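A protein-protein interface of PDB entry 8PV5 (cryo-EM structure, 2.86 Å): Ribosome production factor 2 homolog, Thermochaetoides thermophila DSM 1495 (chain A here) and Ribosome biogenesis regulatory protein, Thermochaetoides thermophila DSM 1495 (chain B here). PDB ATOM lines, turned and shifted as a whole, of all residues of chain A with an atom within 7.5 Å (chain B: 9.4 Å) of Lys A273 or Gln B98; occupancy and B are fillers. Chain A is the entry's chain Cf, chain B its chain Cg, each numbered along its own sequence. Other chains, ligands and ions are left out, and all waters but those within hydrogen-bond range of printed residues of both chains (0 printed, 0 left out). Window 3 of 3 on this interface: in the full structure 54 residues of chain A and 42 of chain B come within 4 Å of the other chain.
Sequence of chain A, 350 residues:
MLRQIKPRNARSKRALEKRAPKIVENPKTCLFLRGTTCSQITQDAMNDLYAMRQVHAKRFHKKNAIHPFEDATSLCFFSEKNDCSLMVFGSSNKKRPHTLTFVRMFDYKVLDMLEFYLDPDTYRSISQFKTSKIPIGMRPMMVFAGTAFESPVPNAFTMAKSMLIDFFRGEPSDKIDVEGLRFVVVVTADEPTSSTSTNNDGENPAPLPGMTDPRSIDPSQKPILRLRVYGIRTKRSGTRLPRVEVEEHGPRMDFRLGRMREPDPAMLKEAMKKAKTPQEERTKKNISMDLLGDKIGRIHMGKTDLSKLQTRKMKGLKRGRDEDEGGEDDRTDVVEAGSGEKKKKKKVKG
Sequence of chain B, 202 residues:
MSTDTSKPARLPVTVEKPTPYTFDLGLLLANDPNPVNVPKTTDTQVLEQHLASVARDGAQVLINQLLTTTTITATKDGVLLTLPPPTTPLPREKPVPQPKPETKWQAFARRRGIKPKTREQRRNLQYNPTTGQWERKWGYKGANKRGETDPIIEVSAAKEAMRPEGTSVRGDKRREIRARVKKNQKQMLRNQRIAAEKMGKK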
ATOM      1  N   PRO A  21     -29.090  30.049  20.636  1.00  0.00           N
ATOM      2  CA  PRO A  21     -28.252  29.061  21.329  1.00  0.00           C
ATOM      3  C   PRO A  21     -26.770  29.325  21.106  1.00  0.00           C
ATOM      4  O   PRO A  21     -26.350  29.759  20.031  1.00  0.00           O
ATOM      5  CB  PRO A  21     -28.686  27.731  20.706  1.00  0.00           C
ATOM      6  CG  PRO A  21     -30.066  27.983  20.214  1.00  0.00           C
ATOM      7  CD  PRO A  21     -30.060  29.403  19.736  1.00  0.00           C
ATOM      8  N   ILE A  23     -22.491  28.077  22.341  1.00  0.00           N
ATOM      9  CA  ILE A  23     -21.636  27.000  22.840  1.00  0.00           C
ATOM     10  C   ILE A  23     -21.500  27.092  24.354  1.00  0.00           C
ATOM     11  O   ILE A  23     -21.681  26.103  25.075  1.00  0.00           O
ATOM     12  CB  ILE A  23     -20.264  27.039  22.144  1.00  0.00           C
ATOM     13  CG1 ILE A  23     -20.416  26.742  20.651  1.00  0.00           C
ATOM     14  CG2 ILE A  23     -19.305  26.052  22.787  1.00  0.00           C
ATOM     15  CD1 ILE A  23     -21.037  25.394  20.360  1.00  0.00           C
ATOM     16  N   PHE A 106     -36.089  23.067  28.895  1.00  0.00           N
ATOM     17  CA  PHE A 106     -35.046  22.796  27.915  1.00  0.00           C
ATOM     18  C   PHE A 106     -35.618  23.058  26.531  1.00  0.00           C
ATOM     19  O   PHE A 106     -36.633  22.458  26.163  1.00  0.00           O
ATOM     20  CB  PHE A 106     -34.516  21.363  27.999  1.00  0.00           C
ATOM     21  CG  PHE A 106     -33.486  21.049  26.952  1.00  0.00           C
ATOM     22  CD1 PHE A 106     -32.215  21.594  27.030  1.00  0.00           C
ATOM     23  CD2 PHE A 106     -33.792  20.226  25.881  1.00  0.00           C
ATOM     24  CE1 PHE A 106     -31.268  21.320  26.063  1.00  0.00           C
ATOM     25  CE2 PHE A 106     -32.847  19.947  24.911  1.00  0.00           C
ATOM     26  CZ  PHE A 106     -31.584  20.493  25.004  1.00  0.00           C
ATOM     27  N   ALA A 266     -34.605  11.111  25.954  1.00  0.00           N
ATOM     28  CA  ALA A 266     -33.888  11.758  24.858  1.00  0.00           C
ATOM     29  C   ALA A 266     -33.658  13.237  25.142  1.00  0.00           C
ATOM     30  O   ALA A 266     -32.571  13.764  24.877  1.00  0.00           O
ATOM     31  CB  ALA A 266     -34.656  11.577  23.549  1.00  0.00           C
ATOM     32  N   MET A 267     -34.665  13.910  25.704  1.00  0.00           N
ATOM     33  CA  MET A 267     -34.497  15.298  26.123  1.00  0.00           C
ATOM     34  C   MET A 267     -33.450  15.417  27.224  1.00  0.00           C
ATOM     35  O   MET A 267     -32.720  16.411  27.291  1.00  0.00           O
ATOM     36  CB  MET A 267     -35.839  15.867  26.586  1.00  0.00           C
ATOM     37  CG  MET A 267     -35.812  17.345  26.935  1.00  0.00           C
ATOM     38  SD  MET A 267     -37.416  17.971  27.464  1.00  0.00           S
ATOM     39  CE  MET A 267     -38.305  17.972  25.911  1.00  0.00           C
ATOM     40  N   LEU A 268     -33.341  14.400  28.082  1.00  0.00           N
ATOM     41  CA  LEU A 268     -32.347  14.435  29.149  1.00  0.00           C
ATOM     42  C   LEU A 268     -30.932  14.322  28.597  1.00  0.00           C
ATOM     43  O   LEU A 268     -30.034  15.045  29.040  1.00  0.00           O
ATOM     44  CB  LEU A 268     -32.618  13.326  30.164  1.00  0.00           C
ATOM     45  CG  LEU A 268     -31.681  13.295  31.371  1.00  0.00           C
ATOM     46  CD1 LEU A 268     -31.823  14.571  32.181  1.00  0.00           C
ATOM     47  CD2 LEU A 268     -31.952  12.076  32.236  1.00  0.00           C
ATOM     48  N   LYS A 269     -30.707  13.422  27.631  1.00  0.00           N
ATOM     49  CA  LYS A 269     -29.385  13.392  26.999  1.00  0.00           C
ATOM     50  C   LYS A 269     -29.101  14.665  26.207  1.00  0.00           C
ATOM     51  O   LYS A 269     -27.960  15.143  26.198  1.00  0.00           O
ATOM     52  CB  LYS A 269     -29.158  12.162  26.109  1.00  0.00           C
ATOM     53  CG  LYS A 269     -28.695  10.888  26.839  1.00  0.00           C
ATOM     54  CD  LYS A 269     -29.721  10.137  27.649  1.00  0.00           C
ATOM     55  CE  LYS A 269     -30.718   9.475  26.720  1.00  0.00           C
ATOM     56  NZ  LYS A 269     -31.710   8.672  27.480  1.00  0.00           N
ATOM     57  N   GLU A 270     -30.112  15.231  25.539  1.00  0.00           N
ATOM     58  CA  GLU A 270     -29.892  16.487  24.821  1.00  0.00           C
ATOM     59  C   GLU A 270     -29.572  17.640  25.767  1.00  0.00           C
ATOM     60  O   GLU A 270     -28.805  18.539  25.407  1.00  0.00           O
ATOM     61  CB  GLU A 270     -31.105  16.829  23.959  1.00  0.00           C
ATOM     62  CG  GLU A 270     -31.313  15.884  22.790  1.00  0.00           C
ATOM     63  CD  GLU A 270     -32.690  16.016  22.172  1.00  0.00           C
ATOM     64  OE1 GLU A 270     -33.545  16.706  22.765  1.00  0.00           O
ATOM     65  OE2 GLU A 270     -32.917  15.427  21.095  1.00  0.00           O
ATOM     66  N   ALA A 271     -30.143  17.632  26.973  1.00  0.00           N
ATOM     67  CA  ALA A 271     -29.817  18.640  27.972  1.00  0.00           C
ATOM     68  C   ALA A 271     -28.471  18.395  28.638  1.00  0.00           C
ATOM     69  O   ALA A 271     -27.809  19.359  29.034  1.00  0.00           O
ATOM     70  CB  ALA A 271     -30.912  18.700  29.039  1.00  0.00           C
ATOM     71  N   MET A 272     -28.058  17.139  28.779  1.00  0.00           N
ATOM     72  CA  MET A 272     -26.785  16.816  29.406  1.00  0.00           C
ATOM     73  C   MET A 272     -25.636  16.725  28.411  1.00  0.00           C
ATOM     74  O   MET A 272     -24.519  16.387  28.815  1.00  0.00           O
ATOM     75  CB  MET A 272     -26.896  15.501  30.182  1.00  0.00           C
ATOM     76  CG  MET A 272     -27.846  15.556  31.364  1.00  0.00           C
ATOM     77  SD  MET A 272     -27.329  16.704  32.649  1.00  0.00           S
ATOM     78  CE  MET A 272     -28.770  16.668  33.708  1.00  0.00           C
ATOM     79  N   LYS A 273     -25.882  16.988  27.128  1.00  0.00           N
ATOM     80  CA  LYS A 273     -24.783  17.188  26.192  1.00  0.00           C
ATOM     81  C   LYS A 273     -23.961  18.403  26.600  1.00  0.00           C
ATOM     82  O   LYS A 273     -24.504  19.471  26.892  1.00  0.00           O
ATOM     83  CB  LYS A 273     -25.308  17.375  24.767  1.00  0.00           C
ATOM     84  CG  LYS A 273     -25.727  16.095  24.069  1.00  0.00           C
ATOM     85  CD  LYS A 273     -26.330  16.385  22.704  1.00  0.00           C
ATOM     86  CE  LYS A 273     -25.276  16.871  21.724  1.00  0.00           C
ATOM     87  NZ  LYS A 273     -25.834  17.047  20.355  1.00  0.00           N
ATOM     88  N   LYS A 274     -22.642  18.236  26.619  1.00  0.00           N
ATOM     89  CA  LYS A 274     -21.723  19.290  27.027  1.00  0.00           C
ATOM     90  C   LYS A 274     -20.947  19.762  25.808  1.00  0.00           C
ATOM     91  O   LYS A 274     -20.182  18.991  25.218  1.00  0.00           O
ATOM     92  CB  LYS A 274     -20.775  18.796  28.121  1.00  0.00           C
ATOM     93  CG  LYS A 274     -19.808  19.848  28.633  1.00  0.00           C
ATOM     94  CD  LYS A 274     -18.999  19.317  29.804  1.00  0.00           C
ATOM     95  CE  LYS A 274     -17.960  18.310  29.341  1.00  0.00           C
ATOM     96  NZ  LYS A 274     -17.081  17.865  30.459  1.00  0.00           N
ATOM     97  N   ALA A 275     -21.146  21.021  25.434  1.00  0.00           N
ATOM     98  CA  ALA A 275     -20.449  21.594  24.295  1.00  0.00           C
ATOM     99  C   ALA A 275     -18.992  21.859  24.647  1.00  0.00           C
ATOM    100  O   ALA A 275     -18.632  22.026  25.814  1.00  0.00           O
ATOM    101  CB  ALA A 275     -21.124  22.889  23.845  1.00  0.00           C
ATOM    102  N   LYS A 276     -18.152  21.897  23.619  1.00  0.00           N
ATOM    103  CA  LYS A 276     -16.721  22.099  23.792  1.00  0.00           C
ATOM    104  C   LYS A 276     -16.355  23.522  23.394  1.00  0.00           C
ATOM    105  O   LYS A 276     -16.712  23.980  22.303  1.00  0.00           O
ATOM    106  CB  LYS A 276     -15.923  21.091  22.963  1.00  0.00           C
ATOM    107  CG  LYS A 276     -14.417  21.215  23.124  1.00  0.00           C
ATOM    108  CD  LYS A 276     -13.686  20.101  22.394  1.00  0.00           C
ATOM    109  CE  LYS A 276     -13.756  20.292  20.888  1.00  0.00           C
ATOM    110  NZ  LYS A 276     -12.971  21.477  20.448  1.00  0.00           N
ATOM    111  N   PRO B  89     -22.631  18.005  36.981  1.00  0.00           N
ATOM    112  CA  PRO B  89     -23.415  18.068  35.739  1.00  0.00           C
ATOM    113  C   PRO B  89     -24.731  18.800  35.954  1.00  0.00           C
ATOM    114  O   PRO B  89     -25.498  18.477  36.865  1.00  0.00           O
ATOM    115  CB  PRO B  89     -23.642  16.592  35.384  1.00  0.00           C
ATOM    116  CG  PRO B  89     -22.659  15.826  36.220  1.00  0.00           C
ATOM    117  CD  PRO B  89     -22.487  16.626  37.467  1.00  0.00           C
ATOM    118  N   LEU B  90     -24.988  19.788  35.104  1.00  0.00           N
ATOM    119  CA  LEU B  90     -26.220  20.557  35.127  1.00  0.00           C
ATOM    120  C   LEU B  90     -26.766  20.643  33.711  1.00  0.00           C
ATOM    121  O   LEU B  90     -25.993  20.759  32.752  1.00  0.00           O
ATOM    122  CB  LEU B  90     -25.999  21.970  35.687  1.00  0.00           C
ATOM    123  CG  LEU B  90     -25.741  22.073  37.191  1.00  0.00           C
ATOM    124  CD1 LEU B  90     -25.185  23.442  37.545  1.00  0.00           C
ATOM    125  CD2 LEU B  90     -27.012  21.790  37.969  1.00  0.00           C
ATOM    126  N   PRO B  91     -28.086  20.583  33.547  1.00  0.00           N
ATOM    127  CA  PRO B  91     -28.657  20.611  32.196  1.00  0.00           C
ATOM    128  C   PRO B  91     -28.562  21.994  31.569  1.00  0.00           C
ATOM    129  O   PRO B  91     -28.614  23.016  32.255  1.00  0.00           O
ATOM    130  CB  PRO B  91     -30.116  20.201  32.421  1.00  0.00           C
ATOM    131  CG  PRO B  91     -30.399  20.593  33.821  1.00  0.00           C
ATOM    132  CD  PRO B  91     -29.121  20.397  34.580  1.00  0.00           C
ATOM    133  N   ARG B  92     -28.420  22.011  30.248  1.00  0.00           N
ATOM    134  CA  ARG B  92     -28.402  23.254  29.499  1.00  0.00           C
ATOM    135  C   ARG B  92     -29.810  23.823  29.380  1.00  0.00           C
ATOM    136  O   ARG B  92     -30.810  23.133  29.589  1.00  0.00           O
ATOM    137  CB  ARG B  92     -27.817  23.036  28.104  1.00  0.00           C
ATOM    138  CG  ARG B  92     -26.312  22.898  28.070  1.00  0.00           C
ATOM    139  CD  ARG B  92     -25.842  22.456  26.695  1.00  0.00           C
ATOM    140  NE  ARG B  92     -26.291  23.347  25.633  1.00  0.00           N
ATOM    141  CZ  ARG B  92     -25.554  24.315  25.109  1.00  0.00           C
ATOM    142  NH1 ARG B  92     -24.322  24.549  25.528  1.00  0.00           N
ATOM    143  NH2 ARG B  92     -26.065  25.066  24.137  1.00  0.00           N
ATOM    144  N   GLU B  93     -29.879  25.106  29.037  1.00  0.00           N
ATOM    145  CA  GLU B  93     -31.162  25.748  28.786  1.00  0.00           C
ATOM    146  C   GLU B  93     -31.571  25.675  27.323  1.00  0.00           C
ATOM    147  O   GLU B  93     -32.757  25.822  27.011  1.00  0.00           O
ATOM    148  CB  GLU B  93     -31.119  27.211  29.241  1.00  0.00           C
ATOM    149  CG  GLU B  93     -30.325  28.140  28.341  1.00  0.00           C
ATOM    150  CD  GLU B  93     -30.413  29.589  28.776  1.00  0.00           C
ATOM    151  OE1 GLU B  93     -30.974  29.852  29.861  1.00  0.00           O
ATOM    152  OE2 GLU B  93     -29.921  30.464  28.035  1.00  0.00           O
ATOM    153  N   LYS B  94     -30.616  25.452  26.426  1.00  0.00           N
ATOM    154  CA  LYS B  94     -30.827  25.360  24.992  1.00  0.00           C
ATOM    155  C   LYS B  94     -29.958  24.245  24.431  1.00  0.00           C
ATOM    156  O   LYS B  94     -28.937  23.896  25.032  1.00  0.00           O
ATOM    157  CB  LYS B  94     -30.488  26.692  24.304  1.00  0.00           C
ATOM    158  CG  LYS B  94     -31.497  27.792  24.577  1.00  0.00           C
ATOM    159  CD  LYS B  94     -30.942  29.160  24.249  1.00  0.00           C
ATOM    160  CE  LYS B  94     -31.891  30.245  24.720  1.00  0.00           C
ATOM    161  NZ  LYS B  94     -31.297  31.601  24.590  1.00  0.00           N
ATOM    162  N   PRO B  95     -30.348  23.648  23.302  1.00  0.00           N
ATOM    163  CA  PRO B  95     -29.516  22.595  22.707  1.00  0.00           C
ATOM    164  C   PRO B  95     -28.191  23.146  22.204  1.00  0.00           C
ATOM    165  O   PRO B  95     -28.065  24.337  21.910  1.00  0.00           O
ATOM    166  CB  PRO B  95     -30.378  22.066  21.554  1.00  0.00           C
ATOM    167  CG  PRO B  95     -31.378  23.137  21.291  1.00  0.00           C
ATOM    168  CD  PRO B  95     -31.645  23.768  22.614  1.00  0.00           C
ATOM    169  N   VAL B  96     -27.194  22.266  22.142  1.00  0.00           N
ATOM    170  CA  VAL B  96     -25.871  22.650  21.637  1.00  0.00           C
ATOM    171  C   VAL B  96     -25.995  23.042  20.172  1.00  0.00           C
ATOM    172  O   VAL B  96     -26.652  22.319  19.395  1.00  0.00           O
ATOM    173  CB  VAL B  96     -24.869  21.497  21.821  1.00  0.00           C
ATOM    174  CG1 VAL B  96     -23.573  21.774  21.080  1.00  0.00           C
ATOM    175  CG2 VAL B  96     -24.594  21.268  23.297  1.00  0.00           C
ATOM    176  N   PRO B  97     -25.448  24.185  19.753  1.00  0.00           N
ATOM    177  CA  PRO B  97     -25.596  24.619  18.357  1.00  0.00           C
ATOM    178  C   PRO B  97     -24.952  23.644  17.382  1.00  0.00           C
ATOM    179  O   PRO B  97     -23.881  23.091  17.639  1.00  0.00           O
ATOM    180  CB  PRO B  97     -24.891  25.980  18.335  1.00  0.00           C
ATOM    181  CG  PRO B  97     -24.940  26.452  19.735  1.00  0.00           C
ATOM    182  CD  PRO B  97     -24.823  25.225  20.586  1.00  0.00           C
ATOM    183  N   GLN B  98     -25.621  23.443  16.257  1.00  0.00           N
ATOM    184  CA  GLN B  98     -25.182  22.570  15.186  1.00  0.00           C
ATOM    185  C   GLN B  98     -24.884  23.414  13.957  1.00  0.00           C
ATOM    186  O   GLN B  98     -25.396  24.534  13.829  1.00  0.00           O
ATOM    187  CB  GLN B  98     -26.257  21.523  14.861  1.00  0.00           C
ATOM    188  CG  GLN B  98     -26.596  20.607  16.024  1.00  0.00           C
ATOM    189  CD  GLN B  98     -25.425  19.743  16.448  1.00  0.00           C
ATOM    190  OE1 GLN B  98     -24.666  19.252  15.612  1.00  0.00           O
ATOM    191  NE2 GLN B  98     -25.271  19.555  17.752  1.00  0.00           N
ATOM    192  N   PRO B  99     -24.021  22.937  13.056  1.00  0.00           N
ATOM    193  CA  PRO B  99     -23.817  23.651  11.791  1.00  0.00           C
ATOM    194  C   PRO B  99     -25.105  23.729  10.987  1.00  0.00           C
ATOM    195  O   PRO B  99     -25.891  22.780  10.942  1.00  0.00           O
ATOM    196  CB  PRO B  99     -22.755  22.810  11.077  1.00  0.00           C
ATOM    197  CG  PRO B  99     -22.024  22.124  12.176  1.00  0.00           C
ATOM    198  CD  PRO B  99     -23.059  21.834  13.223  1.00  0.00           C
ATOM    199  N   LYS B 100     -25.320  24.883  10.362  1.00  0.00           N
ATOM    200  CA  LYS B 100     -26.529  25.105   9.592  1.00  0.00           C
ATOM    201  C   LYS B 100     -26.518  24.238   8.332  1.00  0.00           C
ATOM    202  O   LYS B 100     -25.448  23.853   7.848  1.00  0.00           O
ATOM    203  CB  LYS B 100     -26.655  26.583   9.222  1.00  0.00           C
ATOM    204  CG  LYS B 100     -25.571  27.096   8.287  1.00  0.00           C
ATOM    205  CD  LYS B 100     -25.727  28.586   8.025  1.00  0.00           C
ATOM    206  CE  LYS B 100     -26.947  28.874   7.168  1.00  0.00           C
ATOM    207  NZ  LYS B 100     -26.800  28.330   5.791  1.00  0.00           N
ATOM    208  N   PRO B 101     -27.694  23.867   7.820  1.00  0.00           N
ATOM    209  CA  PRO B 101     -27.741  23.124   6.555  1.00  0.00           C
ATOM    210  C   PRO B 101     -27.163  23.942   5.411  1.00  0.00           C
ATOM    211  O   PRO B 101     -27.344  25.160   5.342  1.00  0.00           O
ATOM    212  CB  PRO B 101     -29.236  22.852   6.358  1.00  0.00           C
ATOM    213  CG  PRO B 101     -29.813  22.919   7.728  1.00  0.00           C
ATOM    214  CD  PRO B 101     -29.023  23.969   8.445  1.00  0.00           C
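Of the printed residues of chain B, Ala A271 touches Pro B91 (3.5 Å) and Arg B92 (3.0 Å).
Lys A273 touches two residues of chain B.
Lys A274 touches none of the printed residues of chain B.
Of the printed residues of chain A, Pro B91 touches Ala A271 (3.5 Å) and Met A272 (3.8 Å).
Printed residues of chain A within 4 Å of Glu B93: Phe A106 (3.9 Å).
Of the printed residues of chain A, Val B96 touches Ala A275 (3.9 Å).
Of the printed residues of chain A, Gln B98 touches Lys A273.
Pro B101 touches none of the printed residues of chain A.
The nearest residue of chain B that does not touch Lys A273 is Val B96 (4.02 Å).
The nearest residue of chain A that does not touch Gln B98 is Ile A23 (6.5 Å).
The nearest printed residue of chain B that does not touch Met A272 is Leu B90 (4.1 Å).
Among the printed residues, pairs that only touch across the chains: Pro A21 with Lys B94, Pro A21 with Pro B95, Pro A21 with Pro B97, Ile A23 with Pro B97, Phe A106 with Arg B92, Phe A106 with Glu B93, Phe A106 with Lys B94, Phe A106 with Pro B95, Ala A271 with Pro B91, Met A272 with Pro B91, Lys A273 with Arg B92, Lys A273 with Gln B98, Ala A275 with Arg B92 and Ala A275 with Val B96.
Printed residues of chain A that touch a printed residue of chain B: Pro A21, Ile A23, Phe A106, Ala A271, Met A272, Lys A273 and Ala A275.
Along chain A the printed residues that touch a printed residue of chain B span positions 21 to 275.
Of the 13 printed residues of chain B, 8 touch a printed residue of chain A.
Printed residues of chain B that touch a printed residue of chain A: Pro B91, Arg B92, Glu B93, Lys B94, Pro B95, Val B96, Pro B97 and Gln B98.
Hydrophobic or aromatic side chains of chain B that line the printed part of chain A: Pro B91, Pro B95, Val B96 and Pro B97.
Among the printed residues, no Asp or Glu carboxylate lies within 4 Å of a Lys or Arg side-chain nitrogen of the other chain.
The backbone carbonyl oxygen (O) of Ala A271 lies within hydrogen-bond range of the backbone NH (N) of Arg B92, 3.0 Å away.
The backbone carbonyl oxygen of Ile A23 lies within hydrogen-bond range of the guanidinium group of Arg B92 (3.1 Å).
NH2 of Arg B92 lies within hydrogen-bond range of O of Pro B95, 3.1 Å away.
The guanidinium group of Arg B92 is in hydrogen-bond range of the backbone carbonyl oxygen of Lys B94.
The backbone carbonyl oxygen of Val B96 lies within hydrogen-bond range of the side-chain amide nitrogen of Gln B98 (3.5 Å).
The side-chain amino group of Lys B94 is in salt-bridge range of the side-chain carboxylate of Glu B93.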
